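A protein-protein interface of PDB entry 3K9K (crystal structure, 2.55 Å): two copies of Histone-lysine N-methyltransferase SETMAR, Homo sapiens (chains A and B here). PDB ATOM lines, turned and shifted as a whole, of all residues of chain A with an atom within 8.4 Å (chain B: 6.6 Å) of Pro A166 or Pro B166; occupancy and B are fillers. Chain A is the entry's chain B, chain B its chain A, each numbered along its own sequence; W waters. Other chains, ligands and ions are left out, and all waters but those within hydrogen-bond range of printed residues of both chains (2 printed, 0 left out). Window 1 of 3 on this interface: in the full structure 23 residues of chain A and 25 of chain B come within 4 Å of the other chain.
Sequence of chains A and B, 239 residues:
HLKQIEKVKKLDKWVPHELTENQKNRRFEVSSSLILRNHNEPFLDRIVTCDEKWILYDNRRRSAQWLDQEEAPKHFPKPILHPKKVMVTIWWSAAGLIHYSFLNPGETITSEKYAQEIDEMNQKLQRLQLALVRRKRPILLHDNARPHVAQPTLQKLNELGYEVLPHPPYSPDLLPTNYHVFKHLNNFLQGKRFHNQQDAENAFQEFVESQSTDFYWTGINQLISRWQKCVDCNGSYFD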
ATOM      1  N   ARG A  26      19.340 -12.737  -3.228  1.00  0.00           N
ATOM      2  CA  ARG A  26      17.925 -12.470  -3.032  1.00  0.00           C
ATOM      3  C   ARG A  26      17.742 -11.541  -1.835  1.00  0.00           C
ATOM      4  O   ARG A  26      16.850 -10.706  -1.830  1.00  0.00           O
ATOM      5  CB  ARG A  26      17.138 -13.768  -2.839  1.00  0.00           C
ATOM      6  CG  ARG A  26      17.370 -14.817  -3.917  1.00  0.00           C
ATOM      7  CD  ARG A  26      16.566 -14.577  -5.197  1.00  0.00           C
ATOM      8  NE  ARG A  26      17.176 -13.603  -6.107  1.00  0.00           N
ATOM      9  CZ  ARG A  26      18.286 -13.818  -6.814  1.00  0.00           C
ATOM     10  NH1 ARG A  26      18.935 -14.973  -6.707  1.00  0.00           N
ATOM     11  NH2 ARG A  26      18.761 -12.872  -7.622  1.00  0.00           N
ATOM     12  N   GLU A  29      19.107  -8.004  -2.945  1.00  0.00           N
ATOM     13  CA  GLU A  29      18.190  -7.452  -3.931  1.00  0.00           C
ATOM     14  C   GLU A  29      16.906  -6.923  -3.304  1.00  0.00           C
ATOM     15  O   GLU A  29      16.426  -5.826  -3.641  1.00  0.00           O
ATOM     16  CB  GLU A  29      17.846  -8.525  -4.961  1.00  0.00           C
ATOM     17  CG  GLU A  29      16.651  -8.195  -5.843  1.00  0.00           C
ATOM     18  CD  GLU A  29      16.208  -9.386  -6.695  1.00  0.00           C
ATOM     19  OE1 GLU A  29      15.117  -9.306  -7.311  1.00  0.00           O
ATOM     20  OE2 GLU A  29      16.949 -10.401  -6.743  1.00  0.00           O
ATOM     21  N   VAL A  30      16.333  -7.712  -2.404  1.00  0.00           N
ATOM     22  CA  VAL A  30      15.108  -7.297  -1.749  1.00  0.00           C
ATOM     23  C   VAL A  30      15.385  -6.155  -0.773  1.00  0.00           C
ATOM     24  O   VAL A  30      14.661  -5.165  -0.720  1.00  0.00           O
ATOM     25  CB  VAL A  30      14.470  -8.466  -1.002  1.00  0.00           C
ATOM     26  CG1 VAL A  30      13.406  -7.951  -0.027  1.00  0.00           C
ATOM     27  CG2 VAL A  30      13.895  -9.456  -1.999  1.00  0.00           C
ATOM     28  N   SER A  31      16.456  -6.291  -0.012  1.00  0.00           N
ATOM     29  CA  SER A  31      16.792  -5.278   0.955  1.00  0.00           C
ATOM     30  C   SER A  31      17.016  -3.965   0.247  1.00  0.00           C
ATOM     31  O   SER A  31      16.424  -2.952   0.607  1.00  0.00           O
ATOM     32  CB  SER A  31      17.999  -5.696   1.771  1.00  0.00           C
ATOM     33  OG  SER A  31      17.646  -6.812   2.574  1.00  0.00           O
ATOM     34  N   SER A  33      15.919  -2.940  -2.646  1.00  0.00           N
ATOM     35  CA  SER A  33      14.692  -2.400  -3.205  1.00  0.00           C
ATOM     36  C   SER A  33      13.733  -1.850  -2.158  1.00  0.00           C
ATOM     37  O   SER A  33      12.989  -0.908  -2.430  1.00  0.00           O
ATOM     38  CB  SER A  33      13.988  -3.445  -4.054  1.00  0.00           C
ATOM     39  OG  SER A  33      14.367  -3.322  -5.410  1.00  0.00           O
ATOM     40  N   LEU A  34      13.725  -2.454  -0.971  1.00  0.00           N
ATOM     41  CA  LEU A  34      12.823  -1.991   0.083  1.00  0.00           C
ATOM     42  C   LEU A  34      13.283  -0.631   0.567  1.00  0.00           C
ATOM     43  O   LEU A  34      12.478   0.308   0.627  1.00  0.00           O
ATOM     44  CB  LEU A  34      12.741  -2.991   1.229  1.00  0.00           C
ATOM     45  CG  LEU A  34      11.988  -4.279   0.854  1.00  0.00           C
ATOM     46  CD1 LEU A  34      12.028  -5.243   1.992  1.00  0.00           C
ATOM     47  CD2 LEU A  34      10.548  -4.000   0.438  1.00  0.00           C
ATOM     48  N   ARG A  37      12.332   1.789  -2.038  1.00  0.00           N
ATOM     49  CA  ARG A  37      10.882   1.957  -2.122  1.00  0.00           C
ATOM     50  C   ARG A  37      10.385   2.882  -1.024  1.00  0.00           C
ATOM     51  O   ARG A  37       9.563   3.775  -1.252  1.00  0.00           O
ATOM     52  CB  ARG A  37      10.146   0.616  -2.040  1.00  0.00           C
ATOM     53  CG  ARG A  37       8.626   0.796  -2.080  1.00  0.00           C
ATOM     54  CD  ARG A  37       7.859  -0.514  -2.215  1.00  0.00           C
ATOM     55  NE  ARG A  37       6.431  -0.274  -2.020  1.00  0.00           N
ATOM     56  CZ  ARG A  37       5.504  -1.221  -1.916  1.00  0.00           C
ATOM     57  NH1 ARG A  37       5.842  -2.501  -2.006  1.00  0.00           N
ATOM     58  NH2 ARG A  37       4.233  -0.877  -1.714  1.00  0.00           N
ATOM     59  N   PHE A  43       6.232   3.432   3.600  1.00  0.00           N
ATOM     60  CA  PHE A  43       5.153   2.472   3.796  1.00  0.00           C
ATOM     61  C   PHE A  43       5.285   1.716   5.127  1.00  0.00           C
ATOM     62  O   PHE A  43       4.455   0.879   5.450  1.00  0.00           O
ATOM     63  CB  PHE A  43       5.113   1.485   2.615  1.00  0.00           C
ATOM     64  CG  PHE A  43       6.358   0.661   2.497  1.00  0.00           C
ATOM     65  CD1 PHE A  43       7.343   0.995   1.584  1.00  0.00           C
ATOM     66  CD2 PHE A  43       6.566  -0.414   3.342  1.00  0.00           C
ATOM     67  CE1 PHE A  43       8.498   0.249   1.492  1.00  0.00           C
ATOM     68  CE2 PHE A  43       7.719  -1.144   3.272  1.00  0.00           C
ATOM     69  CZ  PHE A  43       8.691  -0.820   2.341  1.00  0.00           C
ATOM     70  N   ILE A 139      -0.182  -3.542   4.389  1.00  0.00           N
ATOM     71  CA  ILE A 139       0.795  -4.359   3.688  1.00  0.00           C
ATOM     72  C   ILE A 139       1.244  -5.447   4.645  1.00  0.00           C
ATOM     73  O   ILE A 139       1.574  -5.168   5.798  1.00  0.00           O
ATOM     74  CB  ILE A 139       2.027  -3.522   3.268  1.00  0.00           C
ATOM     75  CG1 ILE A 139       1.642  -2.478   2.230  1.00  0.00           C
ATOM     76  CG2 ILE A 139       3.117  -4.402   2.701  1.00  0.00           C
ATOM     77  CD1 ILE A 139       2.829  -1.837   1.590  1.00  0.00           C
ATOM     78  N   LEU A 140       1.241  -6.689   4.182  1.00  0.00           N
ATOM     79  CA  LEU A 140       1.624  -7.785   5.051  1.00  0.00           C
ATOM     80  C   LEU A 140       3.062  -8.241   4.835  1.00  0.00           C
ATOM     81  O   LEU A 140       3.493  -8.503   3.704  1.00  0.00           O
ATOM     82  CB  LEU A 140       0.691  -8.976   4.878  1.00  0.00           C
ATOM     83  CG  LEU A 140       1.092 -10.147   5.770  1.00  0.00           C
ATOM     84  CD1 LEU A 140       0.590  -9.899   7.178  1.00  0.00           C
ATOM     85  CD2 LEU A 140       0.557 -11.456   5.223  1.00  0.00           C
ATOM     86  N   LEU A 141       3.793  -8.349   5.936  1.00  0.00           N
ATOM     87  CA  LEU A 141       5.135  -8.885   5.915  1.00  0.00           C
ATOM     88  C   LEU A 141       5.138 -10.160   6.751  1.00  0.00           C
ATOM     89  O   LEU A 141       4.886 -10.136   7.966  1.00  0.00           O
ATOM     90  CB  LEU A 141       6.119  -7.849   6.471  1.00  0.00           C
ATOM     91  CG  LEU A 141       7.545  -8.289   6.817  1.00  0.00           C
ATOM     92  CD1 LEU A 141       8.239  -8.867   5.599  1.00  0.00           C
ATOM     93  CD2 LEU A 141       8.347  -7.133   7.385  1.00  0.00           C
ATOM     94  N   HIS A 142       5.400 -11.285   6.099  1.00  0.00           N
ATOM     95  CA  HIS A 142       5.460 -12.563   6.796  1.00  0.00           C
ATOM     96  C   HIS A 142       6.244 -13.567   5.972  1.00  0.00           C
ATOM     97  O   HIS A 142       6.604 -13.288   4.826  1.00  0.00           O
ATOM     98  CB  HIS A 142       4.054 -13.083   7.095  1.00  0.00           C
ATOM     99  CG  HIS A 142       3.339 -13.632   5.898  1.00  0.00           C
ATOM    100  ND1 HIS A 142       3.482 -13.101   4.636  1.00  0.00           N
ATOM    101  CD2 HIS A 142       2.467 -14.660   5.777  1.00  0.00           C
ATOM    102  CE1 HIS A 142       2.732 -13.781   3.786  1.00  0.00           C
ATOM    103  NE2 HIS A 142       2.106 -14.732   4.453  1.00  0.00           N
ATOM    104  N   ASN A 144       6.511 -16.388   3.694  1.00  0.00           N
ATOM    105  CA  ASN A 144       5.606 -16.945   2.696  1.00  0.00           C
ATOM    106  C   ASN A 144       5.943 -18.384   2.374  1.00  0.00           C
ATOM    107  O   ASN A 144       5.220 -19.045   1.628  1.00  0.00           O
ATOM    108  CB  ASN A 144       5.688 -16.122   1.415  1.00  0.00           C
ATOM    109  CG  ASN A 144       7.113 -15.953   0.933  1.00  0.00           C
ATOM    110  OD1 ASN A 144       7.739 -14.915   1.171  1.00  0.00           O
ATOM    111  ND2 ASN A 144       7.649 -16.986   0.280  1.00  0.00           N
ATOM    112  N   GLU A 163      -1.558  -6.217   0.024  1.00  0.00           N
ATOM    113  CA  GLU A 163      -0.334  -6.396  -0.729  1.00  0.00           C
ATOM    114  C   GLU A 163       0.640  -7.132   0.177  1.00  0.00           C
ATOM    115  O   GLU A 163       0.772  -6.785   1.350  1.00  0.00           O
ATOM    116  CB  GLU A 163       0.227  -5.031  -1.125  1.00  0.00           C
ATOM    117  CG  GLU A 163       1.578  -5.097  -1.806  1.00  0.00           C
ATOM    118  CD  GLU A 163       2.188  -3.714  -2.012  1.00  0.00           C
ATOM    119  OE1 GLU A 163       3.445  -3.625  -2.140  1.00  0.00           O
ATOM    120  OE2 GLU A 163       1.399  -2.725  -2.024  1.00  0.00           O
ATOM    121  N   VAL A 164       1.299  -8.163  -0.342  1.00  0.00           N
ATOM    122  CA  VAL A 164       2.323  -8.865   0.429  1.00  0.00           C
ATOM    123  C   VAL A 164       3.705  -8.334   0.044  1.00  0.00           C
ATOM    124  O   VAL A 164       4.040  -8.235  -1.138  1.00  0.00           O
ATOM    125  CB  VAL A 164       2.259 -10.413   0.235  1.00  0.00           C
ATOM    126  CG1 VAL A 164       3.447 -11.113   0.915  1.00  0.00           C
ATOM    127  CG2 VAL A 164       0.933 -10.975   0.750  1.00  0.00           C
ATOM    128  N   LEU A 165       4.496  -7.994   1.057  1.00  0.00           N
ATOM    129  CA  LEU A 165       5.828  -7.430   0.874  1.00  0.00           C
ATOM    130  C   LEU A 165       6.842  -8.500   0.483  1.00  0.00           C
ATOM    131  O   LEU A 165       6.859  -9.578   1.066  1.00  0.00           O
ATOM    132  CB  LEU A 165       6.289  -6.747   2.162  1.00  0.00           C
ATOM    133  CG  LEU A 165       7.353  -5.658   2.064  1.00  0.00           C
ATOM    134  CD1 LEU A 165       6.786  -4.430   1.367  1.00  0.00           C
ATOM    135  CD2 LEU A 165       7.871  -5.286   3.434  1.00  0.00           C
ATOM    136  N   PRO A 166       7.698  -8.202  -0.513  1.00  0.00           N
ATOM    137  CA  PRO A 166       8.757  -9.147  -0.894  1.00  0.00           C
ATOM    138  C   PRO A 166       9.578  -9.514   0.318  1.00  0.00           C
ATOM    139  O   PRO A 166       9.884  -8.639   1.110  1.00  0.00           O
ATOM    140  CB  PRO A 166       9.616  -8.328  -1.868  1.00  0.00           C
ATOM    141  CG  PRO A 166       8.639  -7.375  -2.505  1.00  0.00           C
ATOM    142  CD  PRO A 166       7.665  -7.012  -1.395  1.00  0.00           C
ATOM    143  N   HIS A 167       9.927 -10.783   0.468  1.00  0.00           N
ATOM    144  CA  HIS A 167      10.730 -11.215   1.598  1.00  0.00           C
ATOM    145  C   HIS A 167      11.699 -12.330   1.208  1.00  0.00           C
ATOM    146  O   HIS A 167      11.271 -13.399   0.770  1.00  0.00           O
ATOM    147  CB  HIS A 167       9.834 -11.666   2.764  1.00  0.00           C
ATOM    148  CG  HIS A 167      10.609 -12.192   3.937  1.00  0.00           C
ATOM    149  ND1 HIS A 167      11.413 -11.390   4.714  1.00  0.00           N
ATOM    150  CD2 HIS A 167      10.731 -13.447   4.437  1.00  0.00           C
ATOM    151  CE1 HIS A 167      11.988 -12.122   5.656  1.00  0.00           C
ATOM    152  NE2 HIS A 167      11.584 -13.370   5.511  1.00  0.00           N
ATOM    153  N   PRO A 168      13.013 -12.095   1.379  1.00  0.00           N
ATOM    154  CA  PRO A 168      14.022 -13.060   0.924  1.00  0.00           C
ATOM    155  C   PRO A 168      13.993 -14.326   1.769  1.00  0.00           C
ATOM    156  O   PRO A 168      13.851 -14.237   2.985  1.00  0.00           O
ATOM    157  CB  PRO A 168      15.344 -12.306   1.132  1.00  0.00           C
ATOM    158  CG  PRO A 168      15.032 -11.349   2.240  1.00  0.00           C
ATOM    159  CD  PRO A 168      13.642 -10.875   1.912  1.00  0.00           C
ATOM    160  N   PRO A 169      14.108 -15.496   1.124  1.00  0.00           N
ATOM    161  CA  PRO A 169      14.117 -16.782   1.824  1.00  0.00           C
ATOM    162  C   PRO A 169      15.111 -16.783   2.972  1.00  0.00           C
ATOM    163  O   PRO A 169      16.120 -16.085   2.901  1.00  0.00           O
ATOM    164  CB  PRO A 169      14.572 -17.749   0.735  1.00  0.00           C
ATOM    165  CG  PRO A 169      14.009 -17.156  -0.524  1.00  0.00           C
ATOM    166  CD  PRO A 169      14.079 -15.663  -0.341  1.00  0.00           C
ATOM    167  N   LEU A 174      15.132 -10.335   9.323  1.00  0.00           N
ATOM    168  CA  LEU A 174      14.458  -9.283   8.582  1.00  0.00           C
ATOM    169  C   LEU A 174      12.951  -9.310   8.830  1.00  0.00           C
ATOM    170  O   LEU A 174      12.208  -8.521   8.228  1.00  0.00           O
ATOM    171  CB  LEU A 174      14.732  -9.425   7.082  1.00  0.00           C
ATOM    172  CG  LEU A 174      15.871  -8.652   6.406  1.00  0.00           C
ATOM    173  CD1 LEU A 174      17.157  -8.750   7.169  1.00  0.00           C
ATOM    174  CD2 LEU A 174      16.075  -9.169   4.999  1.00  0.00           C
ATOM    175  N   LEU A 175      12.509 -10.227   9.696  1.00  0.00           N
ATOM    176  CA  LEU A 175      11.125 -10.260  10.178  1.00  0.00           C
ATOM    177  C   LEU A 175      11.084  -9.775  11.612  1.00  0.00           C
ATOM    178  O   LEU A 175      11.616 -10.433  12.501  1.00  0.00           O
ATOM    179  CB  LEU A 175      10.561 -11.669  10.106  1.00  0.00           C
ATOM    180  CG  LEU A 175      10.591 -12.304   8.710  1.00  0.00           C
ATOM    181  CD1 LEU A 175      10.479 -13.827   8.769  1.00  0.00           C
ATOM    182  CD2 LEU A 175       9.520 -11.705   7.808  1.00  0.00           C
ATOM    183  N   TRP A 227      17.671  -3.559   6.673  1.00  0.00           N
ATOM    184  CA  TRP A 227      17.853  -3.656   5.240  1.00  0.00           C
ATOM    185  C   TRP A 227      19.227  -3.116   4.862  1.00  0.00           C
ATOM    186  O   TRP A 227      19.976  -3.749   4.107  1.00  0.00           O
ATOM    187  CB  TRP A 227      16.761  -2.892   4.509  1.00  0.00           C
ATOM    188  CG  TRP A 227      15.415  -3.480   4.702  1.00  0.00           C
ATOM    189  CD1 TRP A 227      15.122  -4.790   4.938  1.00  0.00           C
ATOM    190  CD2 TRP A 227      14.161  -2.785   4.664  1.00  0.00           C
ATOM    191  NE1 TRP A 227      13.759  -4.957   5.053  1.00  0.00           N
ATOM    192  CE2 TRP A 227      13.147  -3.743   4.897  1.00  0.00           C
ATOM    193  CE3 TRP A 227      13.797  -1.451   4.458  1.00  0.00           C
ATOM    194  CZ2 TRP A 227      11.795  -3.404   4.928  1.00  0.00           C
ATOM    195  CZ3 TRP A 227      12.460  -1.122   4.484  1.00  0.00           C
ATOM    196  CH2 TRP A 227      11.473  -2.092   4.716  1.00  0.00           C
ATOM    197  N   VAL B  30       2.495 -12.567  -6.407  1.00  0.00           N
ATOM    198  CA  VAL B  30       3.127 -11.380  -6.974  1.00  0.00           C
ATOM    199  C   VAL B  30       2.138 -10.525  -7.749  1.00  0.00           C
ATOM    200  O   VAL B  30       2.103  -9.300  -7.591  1.00  0.00           O
ATOM    201  CB  VAL B  30       4.293 -11.754  -7.921  1.00  0.00           C
ATOM    202  CG1 VAL B  30       4.908 -10.507  -8.508  1.00  0.00           C
ATOM    203  CG2 VAL B  30       5.355 -12.588  -7.198  1.00  0.00           C
ATOM    204  N   SER B  33      -0.184  -8.791  -5.452  1.00  0.00           N
ATOM    205  CA  SER B  33       0.491  -7.678  -4.803  1.00  0.00           C
ATOM    206  C   SER B  33       0.763  -6.516  -5.763  1.00  0.00           C
ATOM    207  O   SER B  33       0.492  -5.353  -5.442  1.00  0.00           O
ATOM    208  CB  SER B  33       1.772  -8.147  -4.128  1.00  0.00           C
ATOM    209  OG  SER B  33       1.476  -9.126  -3.147  1.00  0.00           O
ATOM    210  N   LEU B  34       1.283  -6.825  -6.948  1.00  0.00           N
ATOM    211  CA  LEU B  34       1.592  -5.779  -7.930  1.00  0.00           C
ATOM    212  C   LEU B  34       0.356  -4.974  -8.355  1.00  0.00           C
ATOM    213  O   LEU B  34       0.401  -3.743  -8.445  1.00  0.00           O
ATOM    214  CB  LEU B  34       2.304  -6.375  -9.144  1.00  0.00           C
ATOM    215  CG  LEU B  34       3.740  -6.843  -8.891  1.00  0.00           C
ATOM    216  CD1 LEU B  34       4.280  -7.688 -10.046  1.00  0.00           C
ATOM    217  CD2 LEU B  34       4.625  -5.653  -8.651  1.00  0.00           C
ATOM    218  N   ARG B  37      -0.493  -2.926  -5.194  1.00  0.00           N
ATOM    219  CA  ARG B  37       0.483  -1.855  -5.043  1.00  0.00           C
ATOM    220  C   ARG B  37       0.289  -0.764  -6.070  1.00  0.00           C
ATOM    221  O   ARG B  37       0.363   0.420  -5.741  1.00  0.00           O
ATOM    222  CB  ARG B  37       1.909  -2.367  -5.150  1.00  0.00           C
ATOM    223  CG  ARG B  37       2.900  -1.236  -5.170  1.00  0.00           C
ATOM    224  CD  ARG B  37       4.308  -1.721  -5.403  1.00  0.00           C
ATOM    225  NE  ARG B  37       5.235  -0.598  -5.513  1.00  0.00           N
ATOM    226  CZ  ARG B  37       6.549  -0.733  -5.646  1.00  0.00           C
ATOM    227  NH1 ARG B  37       7.099  -1.945  -5.690  1.00  0.00           N
ATOM    228  NH2 ARG B  37       7.313   0.345  -5.730  1.00  0.00           N
ATOM    229  N   LEU B 140      13.148  -1.307 -12.365  1.00  0.00           N
ATOM    230  CA  LEU B 140      13.495  -2.343 -13.312  1.00  0.00           C
ATOM    231  C   LEU B 140      12.588  -3.566 -13.178  1.00  0.00           C
ATOM    232  O   LEU B 140      12.429  -4.135 -12.088  1.00  0.00           O
ATOM    233  CB  LEU B 140      14.951  -2.757 -13.131  1.00  0.00           C
ATOM    234  CG  LEU B 140      15.448  -3.818 -14.108  1.00  0.00           C
ATOM    235  CD1 LEU B 140      15.898  -3.172 -15.403  1.00  0.00           C
ATOM    236  CD2 LEU B 140      16.575  -4.652 -13.489  1.00  0.00           C
ATOM    237  N   LEU B 141      11.988  -3.963 -14.297  1.00  0.00           N
ATOM    238  CA  LEU B 141      11.347  -5.270 -14.390  1.00  0.00           C
ATOM    239  C   LEU B 141      12.163  -6.135 -15.344  1.00  0.00           C
ATOM    240  O   LEU B 141      12.334  -5.802 -16.523  1.00  0.00           O
ATOM    241  CB  LEU B 141       9.891  -5.153 -14.849  1.00  0.00           C
ATOM    242  CG  LEU B 141       9.216  -6.481 -15.232  1.00  0.00           C
ATOM    243  CD1 LEU B 141       9.295  -7.521 -14.127  1.00  0.00           C
ATOM    244  CD2 LEU B 141       7.770  -6.220 -15.611  1.00  0.00           C
ATOM    245  N   HIS B 142      12.687  -7.236 -14.828  1.00  0.00           N
ATOM    246  CA  HIS B 142      13.599  -8.047 -15.596  1.00  0.00           C
ATOM    247  C   HIS B 142      13.666  -9.422 -14.961  1.00  0.00           C
ATOM    248  O   HIS B 142      13.068  -9.651 -13.902  1.00  0.00           O
ATOM    249  CB  HIS B 142      14.980  -7.380 -15.630  1.00  0.00           C
ATOM    250  CG  HIS B 142      15.804  -7.622 -14.402  1.00  0.00           C
ATOM    251  ND1 HIS B 142      17.180  -7.713 -14.435  1.00  0.00           N
ATOM    252  CD2 HIS B 142      15.445  -7.814 -13.110  1.00  0.00           C
ATOM    253  CE1 HIS B 142      17.631  -7.948 -13.215  1.00  0.00           C
ATOM    254  NE2 HIS B 142      16.601  -8.016 -12.393  1.00  0.00           N
ATOM    255  N   ASN B 144      15.491 -12.046 -13.009  1.00  0.00           N
ATOM    256  CA  ASN B 144      16.631 -12.261 -12.123  1.00  0.00           C
ATOM    257  C   ASN B 144      17.079 -13.705 -12.134  1.00  0.00           C
ATOM    258  O   ASN B 144      18.086 -14.049 -11.519  1.00  0.00           O
ATOM    259  CB  ASN B 144      16.321 -11.820 -10.693  1.00  0.00           C
ATOM    260  CG  ASN B 144      15.134 -12.547 -10.109  1.00  0.00           C
ATOM    261  OD1 ASN B 144      15.291 -13.525  -9.366  1.00  0.00           O
ATOM    262  ND2 ASN B 144      13.929 -12.086 -10.455  1.00  0.00           N
ATOM    263  N   VAL B 164      13.838  -2.860  -7.860  1.00  0.00           N
ATOM    264  CA  VAL B 164      13.539  -4.035  -8.667  1.00  0.00           C
ATOM    265  C   VAL B 164      12.187  -4.634  -8.295  1.00  0.00           C
ATOM    266  O   VAL B 164      11.966  -5.049  -7.154  1.00  0.00           O
ATOM    267  CB  VAL B 164      14.616  -5.109  -8.511  1.00  0.00           C
ATOM    268  CG1 VAL B 164      14.031  -6.477  -8.764  1.00  0.00           C
ATOM    269  CG2 VAL B 164      15.774  -4.821  -9.449  1.00  0.00           C
ATOM    270  N   LEU B 165      11.286  -4.661  -9.268  1.00  0.00           N
ATOM    271  CA  LEU B 165       9.977  -5.263  -9.100  1.00  0.00           C
ATOM    272  C   LEU B 165      10.139  -6.756  -8.837  1.00  0.00           C
ATOM    273  O   LEU B 165      11.055  -7.390  -9.365  1.00  0.00           O
ATOM    274  CB  LEU B 165       9.153  -5.026 -10.356  1.00  0.00           C
ATOM    275  CG  LEU B 165       7.687  -4.612 -10.246  1.00  0.00           C
ATOM    276  CD1 LEU B 165       7.517  -3.360  -9.399  1.00  0.00           C
ATOM    277  CD2 LEU B 165       7.122  -4.375 -11.644  1.00  0.00           C
ATOM    278  N   PRO B 166       9.272  -7.323  -7.985  1.00  0.00           N
ATOM    279  CA  PRO B 166       9.262  -8.767  -7.714  1.00  0.00           C
ATOM    280  C   PRO B 166       8.921  -9.542  -8.978  1.00  0.00           C
ATOM    281  O   PRO B 166       8.177  -9.045  -9.824  1.00  0.00           O
ATOM    282  CB  PRO B 166       8.119  -8.927  -6.709  1.00  0.00           C
ATOM    283  CG  PRO B 166       7.914  -7.583  -6.130  1.00  0.00           C
ATOM    284  CD  PRO B 166       8.266  -6.601  -7.191  1.00  0.00           C
ATOM    285  N   HIS B 167       9.454 -10.744  -9.119  1.00  0.00           N
ATOM    286  CA  HIS B 167       9.112 -11.546 -10.294  1.00  0.00           C
ATOM    287  C   HIS B 167       9.109 -13.028  -9.984  1.00  0.00           C
ATOM    288  O   HIS B 167      10.100 -13.579  -9.485  1.00  0.00           O
ATOM    289  CB  HIS B 167      10.047 -11.255 -11.475  1.00  0.00           C
ATOM    290  CG  HIS B 167       9.588 -11.852 -12.769  1.00  0.00           C
ATOM    291  ND1 HIS B 167       8.554 -11.317 -13.509  1.00  0.00           N
ATOM    292  CD2 HIS B 167      10.019 -12.939 -13.454  1.00  0.00           C
ATOM    293  CE1 HIS B 167       8.363 -12.053 -14.588  1.00  0.00           C
ATOM    294  NE2 HIS B 167       9.240 -13.041 -14.583  1.00  0.00           N
ATOM    295  N   PRO B 168       7.978 -13.682 -10.278  1.00  0.00           N
ATOM    296  CA  PRO B 168       7.814 -15.122 -10.082  1.00  0.00           C
ATOM    297  C   PRO B 168       8.604 -15.903 -11.142  1.00  0.00           C
ATOM    298  O   PRO B 168       8.664 -15.499 -12.311  1.00  0.00           O
ATOM    299  CB  PRO B 168       6.305 -15.293 -10.272  1.00  0.00           C
ATOM    300  CG  PRO B 168       6.007 -14.293 -11.337  1.00  0.00           C
ATOM    301  CD  PRO B 168       6.759 -13.086 -10.851  1.00  0.00           C
HETATM  302  O   HOH W   1      12.587  -9.323  -8.305  1.00  0.00           O
HETATM  303  O   HOH W   2       6.835  -4.209  -4.665  1.00  0.00           O
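The backbone NH (N) of Val B164 is in hydrogen-bond range of the side-chain hydroxyl (OG) of Ser A33 (2.5 Å).
N of Val A164 sits at hydrogen-bond distance from OG of Ser B33 (3.0 Å).
The side-chain carboxylate (OE2) of Glu A29 is in salt-bridge range of the guanidinium group (NH2) of Arg A26, 3.2 Å away.
N of Leu A140 is in hydrogen-bond range of O of Glu A163.
The guanidinium group (NH1) of Arg A37 lies within salt-bridge range of the side-chain carboxylate (OE1) of Glu A163, at 2.7 Å.
Asn B144 touches Arg A26 (OD1 to NE, 3.8 Å).
OE1 of Glu A29 touches CG1 of Val B164 (3.4 Å).
Arg B37 touches Arg A37.
Glu A163 touches Ser B33 (CG to O, 3.8 Å).
OE2 of Glu A163 touches CB of Arg B37 (3.2 Å).
CG of Pro A166 touches CG of Pro B166, at 3.7 Å.
Printed residues of chain B within 4 Å of Arg A26: Asn B144 (3.8 Å).
Of the printed residues of chain B, Glu A29 touches Val B164.
Printed residues of chain B within 4 Å of Ser A33: Val B164 (2.5 Å).
Printed residues of chain B within 4 Å of Val A164: Ser B33 (3.0 Å).
Of chain B, only Pro B166 comes within 4 Å of Pro A166.
His A167 touches none of the printed residues of chain B.
Of the printed residues of chain A, Ser B33 touches Glu A163 and Val A164.
Leu B140 touches none of the printed residues of chain A.
Of chain A, only Pro A166 comes within 4 Å of Pro B166.
Hydrophobic or aromatic side chains of chain B within 4 Å of the printed part of chain A: Val B164 and Pro B166.
Of the 23 printed residues of chain A, 7 touch a printed residue of chain B.
Along chain A the printed residues that touch a printed residue of chain B span positions 26 to 166.
Among the printed residues, 8 pairs touch across the chains.
Ser A33 touches Val B164, and with the chains exchanged Val A164 touches Ser B33.
Arg B37 touches its own counterpart, Arg A37.
Pro A166 touches its own counterpart, Pro B166.
Of the 8 pairs that touch across the chains among the printed residues, 4 have their exchanged pair printed and touching as well.
Water W2 lies within hydrogen-bond range of NH1 of Arg B37 (2.5 Å) and NH1 of Arg A37 (3.3 Å).
Water W1 bridges O of Leu B165 (2.7 Å) and OE1 of Glu A29 (2.7 Å).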
